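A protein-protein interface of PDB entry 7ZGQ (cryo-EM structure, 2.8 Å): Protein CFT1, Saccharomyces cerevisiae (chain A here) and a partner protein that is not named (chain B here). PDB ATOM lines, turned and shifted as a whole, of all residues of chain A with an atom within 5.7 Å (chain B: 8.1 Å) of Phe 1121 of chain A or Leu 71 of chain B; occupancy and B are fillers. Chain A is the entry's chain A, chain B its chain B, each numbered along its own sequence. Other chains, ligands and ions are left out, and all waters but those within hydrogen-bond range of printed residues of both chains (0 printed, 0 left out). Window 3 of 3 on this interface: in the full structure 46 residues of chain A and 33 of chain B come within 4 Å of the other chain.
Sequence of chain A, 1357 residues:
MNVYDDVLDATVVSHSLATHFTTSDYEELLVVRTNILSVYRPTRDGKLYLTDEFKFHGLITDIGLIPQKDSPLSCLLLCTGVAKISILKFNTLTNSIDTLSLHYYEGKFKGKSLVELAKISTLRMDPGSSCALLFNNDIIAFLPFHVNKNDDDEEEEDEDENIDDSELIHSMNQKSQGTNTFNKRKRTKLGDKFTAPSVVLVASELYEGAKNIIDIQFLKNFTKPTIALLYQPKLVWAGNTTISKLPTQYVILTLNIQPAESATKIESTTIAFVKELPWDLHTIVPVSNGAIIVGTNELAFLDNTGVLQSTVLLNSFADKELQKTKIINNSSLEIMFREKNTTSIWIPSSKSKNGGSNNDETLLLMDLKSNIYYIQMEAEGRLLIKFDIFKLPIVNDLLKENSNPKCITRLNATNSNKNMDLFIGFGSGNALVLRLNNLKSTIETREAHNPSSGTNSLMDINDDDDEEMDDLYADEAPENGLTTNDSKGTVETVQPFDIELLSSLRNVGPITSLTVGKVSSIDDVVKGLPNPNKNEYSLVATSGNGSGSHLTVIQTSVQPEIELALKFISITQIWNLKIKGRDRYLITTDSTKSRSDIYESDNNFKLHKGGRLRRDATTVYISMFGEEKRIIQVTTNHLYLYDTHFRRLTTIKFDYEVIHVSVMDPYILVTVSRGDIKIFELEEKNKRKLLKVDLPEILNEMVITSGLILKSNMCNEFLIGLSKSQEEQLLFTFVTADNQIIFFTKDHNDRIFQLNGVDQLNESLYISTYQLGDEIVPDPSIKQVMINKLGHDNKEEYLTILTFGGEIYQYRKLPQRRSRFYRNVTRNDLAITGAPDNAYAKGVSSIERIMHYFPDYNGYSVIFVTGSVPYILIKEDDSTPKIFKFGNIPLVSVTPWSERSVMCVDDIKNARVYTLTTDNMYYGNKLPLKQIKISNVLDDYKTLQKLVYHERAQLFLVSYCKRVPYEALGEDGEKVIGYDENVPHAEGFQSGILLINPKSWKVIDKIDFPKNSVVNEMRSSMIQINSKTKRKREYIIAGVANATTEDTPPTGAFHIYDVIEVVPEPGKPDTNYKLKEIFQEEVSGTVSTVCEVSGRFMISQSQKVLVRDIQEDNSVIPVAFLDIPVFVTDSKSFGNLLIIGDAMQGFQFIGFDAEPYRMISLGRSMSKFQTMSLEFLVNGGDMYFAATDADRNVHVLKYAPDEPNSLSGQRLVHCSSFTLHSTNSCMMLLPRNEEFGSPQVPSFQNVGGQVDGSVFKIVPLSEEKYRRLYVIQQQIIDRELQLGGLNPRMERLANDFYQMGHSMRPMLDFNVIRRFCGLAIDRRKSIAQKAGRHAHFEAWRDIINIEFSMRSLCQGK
O of Val 1119 of chain A sits close to O of Tyr 87 of chain B (2.8 Å).
Of the 18 printed residues of chain B, 3 touch a printed residue of chain A.
Among the printed residues, 6 pairs touch across the chains.
Among the printed residues, pairs that only touch across the chains: Leu 1106 of chain A with Tyr 87 of chain B, Ala 1120 of chain A with Tyr 87 of chain B, Phe 1121 of chain A with Trp 70 of chain B, Phe 1121 of chain A with Leu 71 of chain B and Phe 1121 of chain A with Tyr 87 of chain B.
The backbone NH (N) of Val 1107 of chain A sits at hydrogen-bond distance from the backbone carbonyl oxygen (O) of Ala 1120 of chain A (3.0 Å).
O of Val 1107 of chain A is in hydrogen-bond range of N of Val 1119 of chain A, 2.7 Å away.
The backbone NH (N) of Trp 70 of chain B is in hydrogen-bond range of the side-chain sulfur (SG) of Cys 67 of chain B (3.3 Å).
Of the printed residues of chain B, Leu 1106 of chain A touches Tyr 87 (3.4 Å).
Of the printed residues of chain B, Val 1119 of chain A touches Tyr 87.
Ala 1120 of chain A touches one residue of chain B.
Phe 1121 of chain A touches just these residues of chain B: Trp 70 (3.4 Å), Leu 71 (3.7 Å) and Tyr 87 (3.7 Å).
Of the printed residues of chain A, Trp 70 of chain B touches Phe 1121 (3.4 Å).
Of the printed residues of chain A, Tyr 87 of chain B touches Leu 1106, Val 1119, Ala 1120 and Phe 1121.
The nearest residue of chain B that does not touch Phe 1121 of chain A is Arg 72 of chain B (5.5 Å).
The nearest residue of chain A that does not touch Leu 71 of chain B is Lys 1104 of chain A (4.3 Å).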
ATOM      1  N   LYS A1104       7.254  -6.802  -4.011  1.00  0.00           N
ATOM      2  CA  LYS A1104       6.763  -6.783  -5.381  1.00  0.00           C
ATOM      3  C   LYS A1104       6.783  -8.190  -5.961  1.00  0.00           C
ATOM      4  O   LYS A1104       7.559  -9.046  -5.532  1.00  0.00           O
ATOM      5  CB  LYS A1104       7.594  -5.854  -6.276  1.00  0.00           C
ATOM      6  CG  LYS A1104       7.210  -4.392  -6.189  1.00  0.00           C
ATOM      7  CD  LYS A1104       7.808  -3.599  -7.337  1.00  0.00           C
ATOM      8  CE  LYS A1104       7.726  -2.106  -7.074  1.00  0.00           C
ATOM      9  NZ  LYS A1104       6.329  -1.670  -6.801  1.00  0.00           N
ATOM     10  N   VAL A1105       5.912  -8.417  -6.943  1.00  0.00           N
ATOM     11  CA  VAL A1105       5.902  -9.637  -7.741  1.00  0.00           C
ATOM     12  C   VAL A1105       5.895  -9.235  -9.210  1.00  0.00           C
ATOM     13  O   VAL A1105       5.114  -8.368  -9.616  1.00  0.00           O
ATOM     14  CB  VAL A1105       4.698 -10.541  -7.412  1.00  0.00           C
ATOM     15  CG1 VAL A1105       4.924 -11.261  -6.092  1.00  0.00           C
ATOM     16  CG2 VAL A1105       3.416  -9.730  -7.355  1.00  0.00           C
ATOM     17  N   LEU A1106       6.767  -9.854 -10.001  1.00  0.00           N
ATOM     18  CA  LEU A1106       6.986  -9.470 -11.389  1.00  0.00           C
ATOM     19  C   LEU A1106       6.803 -10.671 -12.305  1.00  0.00           C
ATOM     20  O   LEU A1106       7.340 -11.749 -12.035  1.00  0.00           O
ATOM     21  CB  LEU A1106       8.387  -8.884 -11.576  1.00  0.00           C
ATOM     22  CG  LEU A1106       8.488  -7.361 -11.574  1.00  0.00           C
ATOM     23  CD1 LEU A1106       9.937  -6.918 -11.513  1.00  0.00           C
ATOM     24  CD2 LEU A1106       7.816  -6.808 -12.807  1.00  0.00           C
ATOM     25  N   VAL A1107       6.060 -10.476 -13.392  1.00  0.00           N
ATOM     26  CA  VAL A1107       5.862 -11.494 -14.417  1.00  0.00           C
ATOM     27  C   VAL A1107       6.691 -11.121 -15.635  1.00  0.00           C
ATOM     28  O   VAL A1107       6.647  -9.975 -16.098  1.00  0.00           O
ATOM     29  CB  VAL A1107       4.378 -11.635 -14.791  1.00  0.00           C
ATOM     30  CG1 VAL A1107       4.209 -12.652 -15.906  1.00  0.00           C
ATOM     31  CG2 VAL A1107       3.581 -12.052 -13.585  1.00  0.00           C
ATOM     32  N   VAL A1119       6.437  -7.926 -17.780  1.00  0.00           N
ATOM     33  CA  VAL A1119       5.215  -7.500 -18.448  1.00  0.00           C
ATOM     34  C   VAL A1119       4.152  -6.994 -17.483  1.00  0.00           C
ATOM     35  O   VAL A1119       3.269  -6.232 -17.907  1.00  0.00           O
ATOM     36  CB  VAL A1119       4.640  -8.631 -19.326  1.00  0.00           C
ATOM     37  CG1 VAL A1119       5.407  -8.730 -20.633  1.00  0.00           C
ATOM     38  CG2 VAL A1119       4.679  -9.955 -18.584  1.00  0.00           C
ATOM     39  N   ALA A1120       4.195  -7.371 -16.209  1.00  0.00           N
ATOM     40  CA  ALA A1120       3.229  -6.887 -15.233  1.00  0.00           C
ATOM     41  C   ALA A1120       3.851  -6.994 -13.850  1.00  0.00           C
ATOM     42  O   ALA A1120       4.840  -7.704 -13.650  1.00  0.00           O
ATOM     43  CB  ALA A1120       1.914  -7.670 -15.303  1.00  0.00           C
ATOM     44  N   PHE A1121       3.261  -6.278 -12.895  1.00  0.00           N
ATOM     45  CA  PHE A1121       3.774  -6.287 -11.533  1.00  0.00           C
ATOM     46  C   PHE A1121       2.648  -5.993 -10.554  1.00  0.00           C
ATOM     47  O   PHE A1121       1.583  -5.495 -10.925  1.00  0.00           O
ATOM     48  CB  PHE A1121       4.915  -5.280 -11.351  1.00  0.00           C
ATOM     49  CG  PHE A1121       4.454  -3.874 -11.103  1.00  0.00           C
ATOM     50  CD1 PHE A1121       4.037  -3.073 -12.150  1.00  0.00           C
ATOM     51  CD2 PHE A1121       4.449  -3.349  -9.821  1.00  0.00           C
ATOM     52  CE1 PHE A1121       3.616  -1.778 -11.924  1.00  0.00           C
ATOM     53  CE2 PHE A1121       4.027  -2.056  -9.589  1.00  0.00           C
ATOM     54  CZ  PHE A1121       3.612  -1.269 -10.642  1.00  0.00           C
ATOM     55  N   LEU A1122       2.904  -6.318  -9.288  1.00  0.00           N
ATOM     56  CA  LEU A1122       1.978  -6.028  -8.203  1.00  0.00           C
ATOM     57  C   LEU A1122       2.772  -5.839  -6.920  1.00  0.00           C
ATOM     58  O   LEU A1122       3.912  -6.291  -6.800  1.00  0.00           O
ATOM     59  CB  LEU A1122       0.936  -7.139  -8.036  1.00  0.00           C
ATOM     60  CG  LEU A1122      -0.337  -6.752  -7.284  1.00  0.00           C
ATOM     61  CD1 LEU A1122      -1.283  -5.977  -8.183  1.00  0.00           C
ATOM     62  CD2 LEU A1122      -1.017  -7.981  -6.714  1.00  0.00           C
ATOM     63  N   ASP A1123       2.153  -5.161  -5.958  1.00  0.00           N
ATOM     64  CA  ASP A1123       2.767  -4.867  -4.671  1.00  0.00           C
ATOM     65  C   ASP A1123       2.160  -5.762  -3.599  1.00  0.00           C
ATOM     66  O   ASP A1123       0.934  -5.891  -3.514  1.00  0.00           O
ATOM     67  CB  ASP A1123       2.578  -3.395  -4.301  1.00  0.00           C
ATOM     68  CG  ASP A1123       3.705  -2.519  -4.806  1.00  0.00           C
ATOM     69  OD1 ASP A1123       4.759  -2.465  -4.141  1.00  0.00           O
ATOM     70  OD2 ASP A1123       3.535  -1.884  -5.869  1.00  0.00           O
ATOM     71  N   MET A1159      -2.262  -7.587 -13.336  1.00  0.00           N
ATOM     72  CA  MET A1159      -2.240  -8.378 -12.106  1.00  0.00           C
ATOM     73  C   MET A1159      -3.420  -8.023 -11.219  1.00  0.00           C
ATOM     74  O   MET A1159      -3.262  -7.651 -10.055  1.00  0.00           O
ATOM     75  CB  MET A1159      -0.936  -8.212 -11.334  1.00  0.00           C
ATOM     76  CG  MET A1159       0.301  -8.453 -12.153  1.00  0.00           C
ATOM     77  SD  MET A1159       1.375  -9.560 -11.227  1.00  0.00           S
ATOM     78  CE  MET A1159       0.770 -11.137 -11.812  1.00  0.00           C
ATOM     79  N   VAL B  66       3.750   4.911 -20.202  1.00  0.00           N
ATOM     80  CA  VAL B  66       3.368   4.364 -18.908  1.00  0.00           C
ATOM     81  C   VAL B  66       3.296   5.486 -17.879  1.00  0.00           C
ATOM     82  O   VAL B  66       3.945   6.533 -18.014  1.00  0.00           O
ATOM     83  CB  VAL B  66       4.343   3.258 -18.462  1.00  0.00           C
ATOM     84  CG1 VAL B  66       4.484   2.207 -19.551  1.00  0.00           C
ATOM     85  CG2 VAL B  66       5.693   3.842 -18.091  1.00  0.00           C
ATOM     86  N   CYS B  67       2.494   5.273 -16.841  1.00  0.00           N
ATOM     87  CA  CYS B  67       2.249   6.288 -15.826  1.00  0.00           C
ATOM     88  C   CYS B  67       3.262   6.139 -14.697  1.00  0.00           C
ATOM     89  O   CYS B  67       3.345   5.080 -14.066  1.00  0.00           O
ATOM     90  CB  CYS B  67       0.824   6.176 -15.285  1.00  0.00           C
ATOM     91  SG  CYS B  67       0.379   7.446 -14.084  1.00  0.00           S
ATOM     92  N   ARG B  68       4.030   7.202 -14.446  1.00  0.00           N
ATOM     93  CA  ARG B  68       4.965   7.187 -13.328  1.00  0.00           C
ATOM     94  C   ARG B  68       4.237   7.112 -11.993  1.00  0.00           C
ATOM     95  O   ARG B  68       4.744   6.503 -11.045  1.00  0.00           O
ATOM     96  CB  ARG B  68       5.862   8.424 -13.376  1.00  0.00           C
ATOM     97  N   HIS B  69       3.054   7.724 -11.901  1.00  0.00           N
ATOM     98  CA  HIS B  69       2.273   7.643 -10.672  1.00  0.00           C
ATOM     99  C   HIS B  69       1.719   6.242 -10.452  1.00  0.00           C
ATOM    100  O   HIS B  69       1.595   5.799  -9.304  1.00  0.00           O
ATOM    101  CB  HIS B  69       1.137   8.666 -10.706  1.00  0.00           C
ATOM    102  CG  HIS B  69       1.605  10.084 -10.805  1.00  0.00           C
ATOM    103  ND1 HIS B  69       0.766  11.123 -11.144  1.00  0.00           N
ATOM    104  CD2 HIS B  69       2.826  10.636 -10.609  1.00  0.00           C
ATOM    105  CE1 HIS B  69       1.448  12.253 -11.152  1.00  0.00           C
ATOM    106  NE2 HIS B  69       2.701  11.986 -10.830  1.00  0.00           N
ATOM    107  N   TRP B  70       1.376   5.536 -11.530  1.00  0.00           N
ATOM    108  CA  TRP B  70       0.905   4.162 -11.396  1.00  0.00           C
ATOM    109  C   TRP B  70       2.036   3.215 -11.023  1.00  0.00           C
ATOM    110  O   TRP B  70       1.809   2.231 -10.311  1.00  0.00           O
ATOM    111  CB  TRP B  70       0.235   3.708 -12.693  1.00  0.00           C
ATOM    112  CG  TRP B  70      -0.336   2.327 -12.632  1.00  0.00           C
ATOM    113  CD1 TRP B  70      -1.503   1.948 -12.037  1.00  0.00           C
ATOM    114  CD2 TRP B  70       0.231   1.140 -13.197  1.00  0.00           C
ATOM    115  NE1 TRP B  70      -1.697   0.597 -12.193  1.00  0.00           N
ATOM    116  CE2 TRP B  70      -0.646   0.079 -12.901  1.00  0.00           C
ATOM    117  CE3 TRP B  70       1.395   0.873 -13.921  1.00  0.00           C
ATOM    118  CZ2 TRP B  70      -0.394  -1.230 -13.305  1.00  0.00           C
ATOM    119  CZ3 TRP B  70       1.642  -0.426 -14.322  1.00  0.00           C
ATOM    120  CH2 TRP B  70       0.752  -1.461 -14.012  1.00  0.00           C
ATOM    121  N   LEU B  71       3.254   3.488 -11.497  1.00  0.00           N
ATOM    122  CA  LEU B  71       4.395   2.655 -11.131  1.00  0.00           C
ATOM    123  C   LEU B  71       4.668   2.722  -9.635  1.00  0.00           C
ATOM    124  O   LEU B  71       4.979   1.704  -9.006  1.00  0.00           O
ATOM    125  CB  LEU B  71       5.631   3.081 -11.922  1.00  0.00           C
ATOM    126  CG  LEU B  71       5.615   2.764 -13.418  1.00  0.00           C
ATOM    127  CD1 LEU B  71       6.850   3.334 -14.097  1.00  0.00           C
ATOM    128  CD2 LEU B  71       5.517   1.265 -13.646  1.00  0.00           C
ATOM    129  N   ARG B  72       4.555   3.911  -9.047  1.00  0.00           N
ATOM    130  CA  ARG B  72       4.739   4.088  -7.613  1.00  0.00           C
ATOM    131  C   ARG B  72       3.482   3.770  -6.815  1.00  0.00           C
ATOM    132  O   ARG B  72       3.511   3.861  -5.583  1.00  0.00           O
ATOM    133  CB  ARG B  72       5.189   5.520  -7.314  1.00  0.00           C
ATOM    134  N   GLY B  73       2.389   3.402  -7.478  1.00  0.00           N
ATOM    135  CA  GLY B  73       1.154   3.103  -6.784  1.00  0.00           C
ATOM    136  C   GLY B  73       0.406   4.308  -6.271  1.00  0.00           C
ATOM    137  O   GLY B  73      -0.409   4.172  -5.353  1.00  0.00           O
ATOM    138  N   LEU B  74       0.653   5.488  -6.835  1.00  0.00           N
ATOM    139  CA  LEU B  74       0.059   6.736  -6.371  1.00  0.00           C
ATOM    140  C   LEU B  74      -0.582   7.489  -7.529  1.00  0.00           C
ATOM    141  O   LEU B  74      -0.409   8.698  -7.692  1.00  0.00           O
ATOM    142  CB  LEU B  74       1.103   7.603  -5.676  1.00  0.00           C
ATOM    143  CG  LEU B  74       1.710   7.002  -4.410  1.00  0.00           C
ATOM    144  CD1 LEU B  74       2.957   7.763  -3.994  1.00  0.00           C
ATOM    145  CD2 LEU B  74       0.682   6.982  -3.292  1.00  0.00           C
ATOM    146  N   CYS B  75      -1.336   6.773  -8.357  1.00  0.00           N
ATOM    147  CA  CYS B  75      -2.060   7.385  -9.462  1.00  0.00           C
ATOM    148  C   CYS B  75      -3.458   7.767  -8.989  1.00  0.00           C
ATOM    149  O   CYS B  75      -4.264   6.894  -8.651  1.00  0.00           O
ATOM    150  CB  CYS B  75      -2.132   6.438 -10.657  1.00  0.00           C
ATOM    151  SG  CYS B  75      -2.647   7.232 -12.200  1.00  0.00           S
ATOM    152  N   LEU B  84      -0.404   5.130 -19.854  1.00  0.00           N
ATOM    153  CA  LEU B  84      -0.678   3.699 -19.864  1.00  0.00           C
ATOM    154  C   LEU B  84      -0.466   3.094 -18.480  1.00  0.00           C
ATOM    155  O   LEU B  84       0.577   3.297 -17.853  1.00  0.00           O
ATOM    156  CB  LEU B  84       0.219   3.003 -20.889  1.00  0.00           C
ATOM    157  CG  LEU B  84       0.142   1.478 -20.987  1.00  0.00           C
ATOM    158  CD1 LEU B  84      -1.294   1.005 -21.033  1.00  0.00           C
ATOM    159  CD2 LEU B  84       0.895   0.988 -22.207  1.00  0.00           C
ATOM    160  N   HIS B  85      -1.461   2.347 -18.006  1.00  0.00           N
ATOM    161  CA  HIS B  85      -1.350   1.610 -16.748  1.00  0.00           C
ATOM    162  C   HIS B  85      -0.987   0.155 -17.042  1.00  0.00           C
ATOM    163  O   HIS B  85      -1.767  -0.777 -16.839  1.00  0.00           O
ATOM    164  CB  HIS B  85      -2.646   1.723 -15.951  1.00  0.00           C
ATOM    165  CG  HIS B  85      -2.831   3.049 -15.283  1.00  0.00           C
ATOM    166  ND1 HIS B  85      -3.896   3.322 -14.454  1.00  0.00           N
ATOM    167  CD2 HIS B  85      -2.085   4.178 -15.323  1.00  0.00           C
ATOM    168  CE1 HIS B  85      -3.799   4.564 -14.011  1.00  0.00           C
ATOM    169  NE2 HIS B  85      -2.709   5.105 -14.524  1.00  0.00           N
ATOM    170  N   GLU B  86       0.237  -0.021 -17.532  1.00  0.00           N
ATOM    171  CA  GLU B  86       0.753  -1.336 -17.883  1.00  0.00           C
ATOM    172  C   GLU B  86       2.272  -1.270 -17.856  1.00  0.00           C
ATOM    173  O   GLU B  86       2.860  -0.282 -18.298  1.00  0.00           O
ATOM    174  CB  GLU B  86       0.254  -1.781 -19.263  1.00  0.00           C
ATOM    175  CG  GLU B  86       0.601  -3.214 -19.626  1.00  0.00           C
ATOM    176  CD  GLU B  86       0.409  -3.500 -21.102  1.00  0.00           C
ATOM    177  OE1 GLU B  86       0.468  -2.547 -21.907  1.00  0.00           O
ATOM    178  OE2 GLU B  86       0.198  -4.678 -21.457  1.00  0.00           O
ATOM    179  N   TYR B  87       2.897  -2.325 -17.340  1.00  0.00           N
ATOM    180  CA  TYR B  87       4.339  -2.339 -17.092  1.00  0.00           C
ATOM    181  C   TYR B  87       5.043  -3.050 -18.244  1.00  0.00           C
ATOM    182  O   TYR B  87       5.294  -4.254 -18.197  1.00  0.00           O
ATOM    183  CB  TYR B  87       4.648  -3.006 -15.757  1.00  0.00           C
ATOM    184  CG  TYR B  87       6.082  -2.839 -15.314  1.00  0.00           C
ATOM    185  CD1 TYR B  87       6.738  -1.625 -15.463  1.00  0.00           C
ATOM    186  CD2 TYR B  87       6.780  -3.896 -14.750  1.00  0.00           C
ATOM    187  CE1 TYR B  87       8.049  -1.467 -15.061  1.00  0.00           C
ATOM    188  CE2 TYR B  87       8.093  -3.747 -14.345  1.00  0.00           C
ATOM    189  CZ  TYR B  87       8.722  -2.533 -14.502  1.00  0.00           C
ATOM    190  OH  TYR B  87      10.029  -2.384 -14.098  1.00  0.00           O
ATOM    191  N   ASN B  88       5.376  -2.290 -19.286  1.00  0.00           N
ATOM    192  CA  ASN B  88       6.216  -2.773 -20.375  1.00  0.00           C
ATOM    193  C   ASN B  88       7.370  -1.799 -20.558  1.00  0.00           C
ATOM    194  O   ASN B  88       7.150  -0.597 -20.737  1.00  0.00           O
ATOM    195  CB  ASN B  88       5.416  -2.938 -21.669  1.00  0.00           C
ATOM    196  CG  ASN B  88       4.631  -1.698 -22.035  1.00  0.00           C
ATOM    197  OD1 ASN B  88       4.338  -0.858 -21.183  1.00  0.00           O
ATOM    198  ND2 ASN B  88       4.276  -1.579 -23.308  1.00  0.00           N
ATOM    199  N   LEU B  89       8.597  -2.320 -20.512  1.00  0.00           N
ATOM    200  CA  LEU B  89       9.793  -1.484 -20.502  1.00  0.00           C
ATOM    201  C   LEU B  89      10.075  -0.812 -21.839  1.00  0.00           C
ATOM    202  O   LEU B  89      10.923   0.085 -21.889  1.00  0.00           O
ATOM    203  CB  LEU B  89      11.005  -2.320 -20.089  1.00  0.00           C
ATOM    204  CG  LEU B  89      10.973  -2.938 -18.691  1.00  0.00           C
ATOM    205  CD1 LEU B  89      12.320  -3.559 -18.352  1.00  0.00           C
ATOM    206  CD2 LEU B  89      10.582  -1.900 -17.653  1.00  0.00           C
ATOM    207  N   MET B  92       8.759   3.126 -21.724  1.00  0.00           N
ATOM    208  CA  MET B  92       8.905   3.913 -20.511  1.00  0.00           C
ATOM    209  C   MET B  92       9.472   5.291 -20.852  1.00  0.00           C
ATOM    210  O   MET B  92      10.513   5.385 -21.512  1.00  0.00           O
ATOM    211  CB  MET B  92       9.818   3.199 -19.514  1.00  0.00           C
ATOM    212  N   PRO B  93       8.802   6.381 -20.439  1.00  0.00           N
ATOM    213  CA  PRO B  93       9.206   7.780 -20.605  1.00  0.00           C
ATOM    214  C   PRO B  93      10.700   8.022 -20.405  1.00  0.00           C
ATOM    215  O   PRO B  93      11.276   7.462 -19.472  1.00  0.00           O
ATOM    216  CB  PRO B  93       8.399   8.500 -19.511  1.00  0.00           C
ATOM    217  CG  PRO B  93       7.382   7.457 -18.993  1.00  0.00           C
ATOM    218  CD  PRO B  93       7.414   6.325 -19.967  1.00  0.00           C
